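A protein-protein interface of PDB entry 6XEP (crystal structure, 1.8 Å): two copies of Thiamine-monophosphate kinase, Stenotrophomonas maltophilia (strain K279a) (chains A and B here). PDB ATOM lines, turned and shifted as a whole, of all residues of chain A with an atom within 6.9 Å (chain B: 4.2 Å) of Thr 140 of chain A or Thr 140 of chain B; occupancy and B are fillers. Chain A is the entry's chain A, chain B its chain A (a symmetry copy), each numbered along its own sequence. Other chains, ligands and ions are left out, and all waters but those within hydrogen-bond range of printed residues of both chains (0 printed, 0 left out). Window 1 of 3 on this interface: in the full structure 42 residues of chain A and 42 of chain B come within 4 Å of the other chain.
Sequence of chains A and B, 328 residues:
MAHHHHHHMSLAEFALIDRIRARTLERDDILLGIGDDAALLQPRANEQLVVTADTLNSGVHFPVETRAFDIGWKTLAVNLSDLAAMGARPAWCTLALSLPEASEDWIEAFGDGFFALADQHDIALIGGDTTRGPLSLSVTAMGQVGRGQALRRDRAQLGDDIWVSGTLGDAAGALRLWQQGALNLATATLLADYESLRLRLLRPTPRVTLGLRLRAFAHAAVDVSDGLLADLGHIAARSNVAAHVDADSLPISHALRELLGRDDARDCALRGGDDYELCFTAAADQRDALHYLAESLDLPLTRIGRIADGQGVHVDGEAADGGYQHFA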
ATOM      1  N   VAL A  51      13.563   1.682   7.688  1.00  0.00           N
ATOM      2  CA  VAL A  51      12.454   2.554   7.348  1.00  0.00           C
ATOM      3  C   VAL A  51      12.987   3.967   7.226  1.00  0.00           C
ATOM      4  O   VAL A  51      13.769   4.414   8.078  1.00  0.00           O
ATOM      5  CB  VAL A  51      11.341   2.492   8.408  1.00  0.00           C
ATOM      6  CG1 VAL A  51      10.197   3.360   7.993  1.00  0.00           C
ATOM      7  CG2 VAL A  51      10.872   1.056   8.598  1.00  0.00           C
ATOM      8  N   THR A  52      12.574   4.660   6.172  1.00  0.00           N
ATOM      9  CA  THR A  52      12.944   6.044   5.925  1.00  0.00           C
ATOM     10  C   THR A  52      11.683   6.870   5.759  1.00  0.00           C
ATOM     11  O   THR A  52      10.649   6.355   5.345  1.00  0.00           O
ATOM     12  CB  THR A  52      13.804   6.205   4.661  1.00  0.00           C
ATOM     13  OG1 THR A  52      13.024   5.895   3.504  1.00  0.00           O
ATOM     14  CG2 THR A  52      15.001   5.294   4.704  1.00  0.00           C
ATOM     15  N   ALA A  53      11.777   8.161   6.070  1.00  0.00           N
ATOM     16  CA  ALA A  53      10.613   9.019   5.914  1.00  0.00           C
ATOM     17  C   ALA A  53      11.103  10.410   5.571  1.00  0.00           C
ATOM     18  O   ALA A  53      12.068  10.887   6.162  1.00  0.00           O
ATOM     19  CB  ALA A  53       9.751   9.078   7.178  1.00  0.00           C
ATOM     20  N   ASP A  54      10.424  11.047   4.624  1.00  0.00           N
ATOM     21  CA  ASP A  54      10.779  12.383   4.160  1.00  0.00           C
ATOM     22  C   ASP A  54       9.492  13.109   3.818  1.00  0.00           C
ATOM     23  O   ASP A  54       8.548  12.494   3.317  1.00  0.00           O
ATOM     24  CB  ASP A  54      11.684  12.332   2.924  1.00  0.00           C
ATOM     25  CG  ASP A  54      13.034  11.688   3.204  1.00  0.00           C
ATOM     26  OD1 ASP A  54      13.172  10.474   2.933  1.00  0.00           O
ATOM     27  OD2 ASP A  54      13.956  12.390   3.701  1.00  0.00           O
ATOM     28  N   LEU A  76       9.100  10.249  -4.050  1.00  0.00           N
ATOM     29  CA  LEU A  76       9.574   8.885  -3.844  1.00  0.00           C
ATOM     30  C   LEU A  76      11.092   8.781  -4.010  1.00  0.00           C
ATOM     31  O   LEU A  76      11.744   8.022  -3.286  1.00  0.00           O
ATOM     32  CB  LEU A  76       8.869   7.936  -4.808  1.00  0.00           C
ATOM     33  CG  LEU A  76       9.291   6.467  -4.786  1.00  0.00           C
ATOM     34  CD1 LEU A  76       9.055   5.837  -3.396  1.00  0.00           C
ATOM     35  CD2 LEU A  76       8.510   5.712  -5.863  1.00  0.00           C
ATOM     36  N   ASN A  79      13.249   9.140  -0.876  1.00  0.00           N
ATOM     37  CA  ASN A  79      13.243   7.989   0.022  1.00  0.00           C
ATOM     38  C   ASN A  79      14.039   6.827  -0.544  1.00  0.00           C
ATOM     39  O   ASN A  79      14.730   6.113   0.197  1.00  0.00           O
ATOM     40  CB  ASN A  79      11.805   7.561   0.280  1.00  0.00           C
ATOM     41  CG  ASN A  79      11.096   8.504   1.194  1.00  0.00           C
ATOM     42  OD1 ASN A  79      10.550   9.520   0.759  1.00  0.00           O
ATOM     43  ND2 ASN A  79      11.124   8.202   2.484  1.00  0.00           N
ATOM     44  N   TRP A  92       8.053  -1.746   0.424  1.00  0.00           N
ATOM     45  CA  TRP A  92       6.730  -1.144   0.541  1.00  0.00           C
ATOM     46  C   TRP A  92       6.861   0.337   0.884  1.00  0.00           C
ATOM     47  O   TRP A  92       7.881   0.791   1.413  1.00  0.00           O
ATOM     48  CB  TRP A  92       5.888  -1.841   1.615  1.00  0.00           C
ATOM     49  CG  TRP A  92       6.027  -3.327   1.665  1.00  0.00           C
ATOM     50  CD1 TRP A  92       5.616  -4.215   0.713  1.00  0.00           C
ATOM     51  CD2 TRP A  92       6.561  -4.115   2.741  1.00  0.00           C
ATOM     52  NE1 TRP A  92       5.876  -5.504   1.117  1.00  0.00           N
ATOM     53  CE2 TRP A  92       6.467  -5.471   2.351  1.00  0.00           C
ATOM     54  CE3 TRP A  92       7.126  -3.808   3.979  1.00  0.00           C
ATOM     55  CZ2 TRP A  92       6.908  -6.517   3.159  1.00  0.00           C
ATOM     56  CZ3 TRP A  92       7.567  -4.854   4.791  1.00  0.00           C
ATOM     57  CH2 TRP A  92       7.460  -6.191   4.367  1.00  0.00           C
ATOM     58  N   CYS A  93       5.809   1.102   0.594  1.00  0.00           N
ATOM     59  CA  CYS A  93       5.805   2.485   1.053  1.00  0.00           C
ATOM     60  C   CYS A  93       4.390   2.962   1.341  1.00  0.00           C
ATOM     61  O   CYS A  93       3.398   2.368   0.903  1.00  0.00           O
ATOM     62  CB  CYS A  93       6.487   3.414   0.044  1.00  0.00           C
ATOM     63  SG  CYS A  93       5.698   3.478  -1.539  1.00  0.00           S
ATOM     64  N   THR A  94       4.309   4.052   2.106  1.00  0.00           N
ATOM     65  CA  THR A  94       3.050   4.747   2.344  1.00  0.00           C
ATOM     66  C   THR A  94       3.185   6.174   1.841  1.00  0.00           C
ATOM     67  O   THR A  94       4.284   6.708   1.708  1.00  0.00           O
ATOM     68  CB  THR A  94       2.661   4.779   3.822  1.00  0.00           C
ATOM     69  OG1 THR A  94       3.683   5.443   4.563  1.00  0.00           O
ATOM     70  CG2 THR A  94       2.434   3.350   4.367  1.00  0.00           C
ATOM     71  N   LEU A  95       2.043   6.777   1.549  1.00  0.00           N
ATOM     72  CA  LEU A  95       2.008   8.131   1.014  1.00  0.00           C
ATOM     73  C   LEU A  95       0.933   8.896   1.755  1.00  0.00           C
ATOM     74  O   LEU A  95      -0.227   8.486   1.740  1.00  0.00           O
ATOM     75  CB  LEU A  95       1.702   8.104  -0.480  1.00  0.00           C
ATOM     76  CG  LEU A  95       1.403   9.412  -1.189  1.00  0.00           C
ATOM     77  CD1 LEU A  95       2.646  10.282  -1.227  1.00  0.00           C
ATOM     78  CD2 LEU A  95       0.925   9.064  -2.573  1.00  0.00           C
ATOM     79  N   ALA A  96       1.312  10.010   2.379  1.00  0.00           N
ATOM     80  CA  ALA A  96       0.386  10.866   3.110  1.00  0.00           C
ATOM     81  C   ALA A  96       0.371  12.206   2.388  1.00  0.00           C
ATOM     82  O   ALA A  96       1.357  12.954   2.443  1.00  0.00           O
ATOM     83  CB  ALA A  96       0.803  11.008   4.575  1.00  0.00           C
ATOM     84  N   ILE A 123       8.977  -1.216  -5.636  1.00  0.00           N
ATOM     85  CA  ILE A 123       8.465  -0.785  -4.337  1.00  0.00           C
ATOM     86  C   ILE A 123       6.968  -0.541  -4.489  1.00  0.00           C
ATOM     87  O   ILE A 123       6.526   0.094  -5.455  1.00  0.00           O
ATOM     88  CB  ILE A 123       9.211   0.451  -3.790  1.00  0.00           C
ATOM     89  CG1 ILE A 123       8.752   0.737  -2.349  1.00  0.00           C
ATOM     90  CG2 ILE A 123       9.010   1.694  -4.673  1.00  0.00           C
ATOM     91  CD1 ILE A 123       9.511   1.900  -1.621  1.00  0.00           C
ATOM     92  N   LEU A 125       3.328   0.833  -3.236  1.00  0.00           N
ATOM     93  CA  LEU A 125       2.511   1.684  -2.377  1.00  0.00           C
ATOM     94  C   LEU A 125       1.419   0.827  -1.742  1.00  0.00           C
ATOM     95  O   LEU A 125       0.634   0.205  -2.460  1.00  0.00           O
ATOM     96  CB  LEU A 125       1.906   2.824  -3.199  1.00  0.00           C
ATOM     97  CG  LEU A 125       0.975   3.815  -2.495  1.00  0.00           C
ATOM     98  CD1 LEU A 125       1.667   4.543  -1.332  1.00  0.00           C
ATOM     99  CD2 LEU A 125       0.477   4.841  -3.512  1.00  0.00           C
ATOM    100  N   SER A 138       4.296  13.380   2.313  1.00  0.00           N
ATOM    101  CA  SER A 138       5.147  12.661   3.250  1.00  0.00           C
ATOM    102  C   SER A 138       5.146  11.191   2.861  1.00  0.00           C
ATOM    103  O   SER A 138       4.086  10.562   2.816  1.00  0.00           O
ATOM    104  CB  SER A 138       4.655  12.834   4.685  1.00  0.00           C
ATOM    105  OG  SER A 138       5.655  12.432   5.609  1.00  0.00           O
ATOM    106  N   VAL A 139       6.326  10.643   2.583  1.00  0.00           N
ATOM    107  CA  VAL A 139       6.443   9.251   2.175  1.00  0.00           C
ATOM    108  C   VAL A 139       7.278   8.513   3.206  1.00  0.00           C
ATOM    109  O   VAL A 139       8.295   9.019   3.692  1.00  0.00           O
ATOM    110  CB  VAL A 139       7.053   9.087   0.770  1.00  0.00           C
ATOM    111  CG1 VAL A 139       7.468   7.624   0.530  1.00  0.00           C
ATOM    112  CG2 VAL A 139       6.059   9.473  -0.272  1.00  0.00           C
ATOM    113  N   THR A 140       6.814   7.330   3.573  1.00  0.00           N
ATOM    114  CA  THR A 140       7.576   6.414   4.395  1.00  0.00           C
ATOM    115  C   THR A 140       7.883   5.219   3.519  1.00  0.00           C
ATOM    116  O   THR A 140       6.964   4.638   2.942  1.00  0.00           O
ATOM    117  CB  THR A 140       6.787   5.994   5.632  1.00  0.00           C
ATOM    118  OG1 THR A 140       6.462   7.157   6.390  1.00  0.00           O
ATOM    119  CG2 THR A 140       7.614   5.088   6.520  1.00  0.00           C
ATOM    120  N   ALA A 141       9.161   4.872   3.402  1.00  0.00           N
ATOM    121  CA  ALA A 141       9.569   3.746   2.577  1.00  0.00           C
ATOM    122  C   ALA A 141      10.240   2.692   3.446  1.00  0.00           C
ATOM    123  O   ALA A 141      11.069   3.005   4.304  1.00  0.00           O
ATOM    124  CB  ALA A 141      10.501   4.189   1.464  1.00  0.00           C
ATOM    125  N   MET A 142       9.870   1.439   3.220  1.00  0.00           N
ATOM    126  CA  MET A 142      10.377   0.304   3.980  1.00  0.00           C
ATOM    127  C   MET A 142      11.204  -0.571   3.053  1.00  0.00           C
ATOM    128  O   MET A 142      10.720  -0.967   1.992  1.00  0.00           O
ATOM    129  CB  MET A 142       9.234  -0.523   4.578  1.00  0.00           C
ATOM    130  CG  MET A 142       8.562   0.084   5.797  1.00  0.00           C
ATOM    131  SD  MET A 142       6.763   0.034   5.661  1.00  0.00           S
ATOM    132  CE  MET A 142       6.560   1.225   4.357  1.00  0.00           C
ATOM    133  N   VAL B  51       0.114  -1.383   8.284  1.00  0.00           N
ATOM    134  CA  VAL B  51       0.711  -0.061   8.349  1.00  0.00           C
ATOM    135  C   VAL B  51      -0.391   0.962   8.165  1.00  0.00           C
ATOM    136  O   VAL B  51      -1.242   0.809   7.276  1.00  0.00           O
ATOM    137  CB  VAL B  51       1.796   0.121   7.273  1.00  0.00           C
ATOM    138  CG1 VAL B  51       2.422   1.472   7.410  1.00  0.00           C
ATOM    139  CG2 VAL B  51       2.854  -0.966   7.400  1.00  0.00           C
ATOM    140  N   THR B  52      -0.380   1.992   9.003  1.00  0.00           N
ATOM    141  CA  THR B  52      -1.329   3.090   8.939  1.00  0.00           C
ATOM    142  C   THR B  52      -0.566   4.397   8.836  1.00  0.00           C
ATOM    143  O   THR B  52       0.565   4.498   9.302  1.00  0.00           O
ATOM    144  CB  THR B  52      -2.241   3.152  10.174  1.00  0.00           C
ATOM    145  OG1 THR B  52      -1.468   3.494  11.327  1.00  0.00           O
ATOM    146  CG2 THR B  52      -2.917   1.828  10.411  1.00  0.00           C
ATOM    147  N   ALA B  53      -1.196   5.405   8.237  1.00  0.00           N
ATOM    148  CA  ALA B  53      -0.533   6.694   8.124  1.00  0.00           C
ATOM    149  C   ALA B  53      -1.599   7.770   8.156  1.00  0.00           C
ATOM    150  O   ALA B  53      -2.642   7.625   7.524  1.00  0.00           O
ATOM    151  CB  ALA B  53       0.284   6.825   6.836  1.00  0.00           C
ATOM    152  N   CYS B  93       6.943   3.160  14.881  1.00  0.00           N
ATOM    153  CA  CYS B  93       6.368   4.256  14.111  1.00  0.00           C
ATOM    154  C   CYS B  93       7.448   5.219  13.641  1.00  0.00           C
ATOM    155  O   CYS B  93       8.573   5.239  14.152  1.00  0.00           O
ATOM    156  CB  CYS B  93       5.296   5.002  14.909  1.00  0.00           C
ATOM    157  SG  CYS B  93       5.889   5.772  16.388  1.00  0.00           S
ATOM    158  N   THR B  94       7.086   6.022  12.640  1.00  0.00           N
ATOM    159  CA  THR B  94       7.927   7.119  12.177  1.00  0.00           C
ATOM    160  C   THR B  94       7.156   8.418  12.337  1.00  0.00           C
ATOM    161  O   THR B  94       5.928   8.434  12.401  1.00  0.00           O
ATOM    162  CB  THR B  94       8.344   6.971  10.713  1.00  0.00           C
ATOM    163  OG1 THR B  94       7.176   6.927   9.894  1.00  0.00           O
ATOM    164  CG2 THR B  94       9.201   5.701  10.507  1.00  0.00           C
ATOM    165  N   VAL B 139       2.426  10.756  10.741  1.00  0.00           N
ATOM    166  CA  VAL B 139       2.905   9.592  11.470  1.00  0.00           C
ATOM    167  C   VAL B 139       2.534   8.345  10.688  1.00  0.00           C
ATOM    168  O   VAL B 139       1.427   8.227  10.153  1.00  0.00           O
ATOM    169  CB  VAL B 139       2.352   9.513  12.905  1.00  0.00           C
ATOM    170  CG1 VAL B 139       2.604   8.118  13.503  1.00  0.00           C
ATOM    171  CG2 VAL B 139       3.020  10.526  13.771  1.00  0.00           C
ATOM    172  N   THR B 140       3.487   7.434  10.584  1.00  0.00           N
ATOM    173  CA  THR B 140       3.247   6.113  10.042  1.00  0.00           C
ATOM    174  C   THR B 140       3.445   5.146  11.189  1.00  0.00           C
ATOM    175  O   THR B 140       4.492   5.177  11.835  1.00  0.00           O
ATOM    176  CB  THR B 140       4.207   5.802   8.897  1.00  0.00           C
ATOM    177  OG1 THR B 140       4.033   6.776   7.870  1.00  0.00           O
ATOM    178  CG2 THR B 140       3.907   4.446   8.293  1.00  0.00           C
ATOM    179  N   ALA B 141       2.442   4.315  11.455  1.00  0.00           N
ATOM    180  CA  ALA B 141       2.521   3.352  12.541  1.00  0.00           C
ATOM    181  C   ALA B 141       2.426   1.940  11.983  1.00  0.00           C
ATOM    182  O   ALA B 141       1.592   1.648  11.122  1.00  0.00           O
ATOM    183  CB  ALA B 141       1.430   3.592  13.570  1.00  0.00           C
ATOM    184  N   MET B 142       3.292   1.066  12.475  1.00  0.00           N
ATOM    185  CA  MET B 142       3.373  -0.320  12.032  1.00  0.00           C
ATOM    186  C   MET B 142       2.962  -1.223  13.182  1.00  0.00           C
ATOM    187  O   MET B 142       3.511  -1.108  14.278  1.00  0.00           O
ATOM    188  CB  MET B 142       4.793  -0.680  11.583  1.00  0.00           C
ATOM    189  CG  MET B 142       5.199  -0.146  10.220  1.00  0.00           C
ATOM    190  SD  MET B 142       6.829   0.627  10.266  1.00  0.00           S
ATOM    191  CE  MET B 142       6.421   2.057  11.241  1.00  0.00           C
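Among the printed residues, pairs that only touch across the chains: Thr 94 of chain A with Val 51 of chain B (3.6 Å), Val 51 of chain A with Thr 94 of chain B (3.6 Å), Thr 94 of chain A with Thr 140 of chain B (3.6 Å) and Thr 140 of chain A with Thr 94 of chain B (3.6 Å).
Val 51 of chain A touches Thr 94 of chain B, and with the chains exchanged Thr 94 of chain A touches Val 51 of chain B. Thr 94 of chain A touches Thr 140 of chain B, and with the chains exchanged Thr 140 of chain A touches Thr 94 of chain B. Thr 140 of chain A touches its own counterpart, Thr 140 of chain B. Of the 5 pairs that touch across the chains among the printed residues, 5 have their exchanged pair printed and touching as well.
The side-chain hydroxyl (OG1) of Thr 140 of chain A sits at hydrogen-bond distance from the side-chain hydroxyl (OG1) of Thr 140 of chain B (2.9 Å).
Of chain B, only Thr 94 (3.6 Å) and Thr 140 (2.9 Å) come within 4 Å of Thr 140 of chain A. Thr 140 of chain B touches two residues of chain A. Printed residues of chain B within 4 Å of Val 51 of chain A: Thr 94 (3.6 Å). Printed residues of chain B within 4 Å of Thr 94 of chain A: Val 51 and Thr 140. Of the printed residues of chain A, Val 51 of chain B touches Thr 94 (3.6 Å). Ala 96 of chain A touches none of the printed residues of chain B. Trp 92 of chain A touches none of the printed residues of chain B. The nearest printed residue of chain B that does not touch Thr 140 of chain A is Met 142 of chain B (5.7 Å).
Of the 9 printed residues of chain B, 3 touch a printed residue of chain A. Hydrophobic or aromatic side chains of chain B within 4 Å of the printed part of chain A: Val 51. Of the 18 printed residues of chain A, 3 touch a printed residue of chain B. Hydrophobic or aromatic side chains of chain A within 4 Å of the printed part of chain B: Val 51. Along chain A the printed residues that touch a printed residue of chain B span positions 51 to 140. Among the printed residues, 5 pairs touch across the chains. Among the printed residues, no Asp or Glu carboxylate lies within 4 Å of a Lys or Arg side-chain nitrogen of the other chain.
N of Thr 94 of chain A lies within hydrogen-bond range of O of Thr 140 of chain A (2.8 Å). The backbone carbonyl oxygen of Thr 140 of chain B sits at hydrogen-bond distance from the backbone NH of Thr 94 of chain B (2.8 Å).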
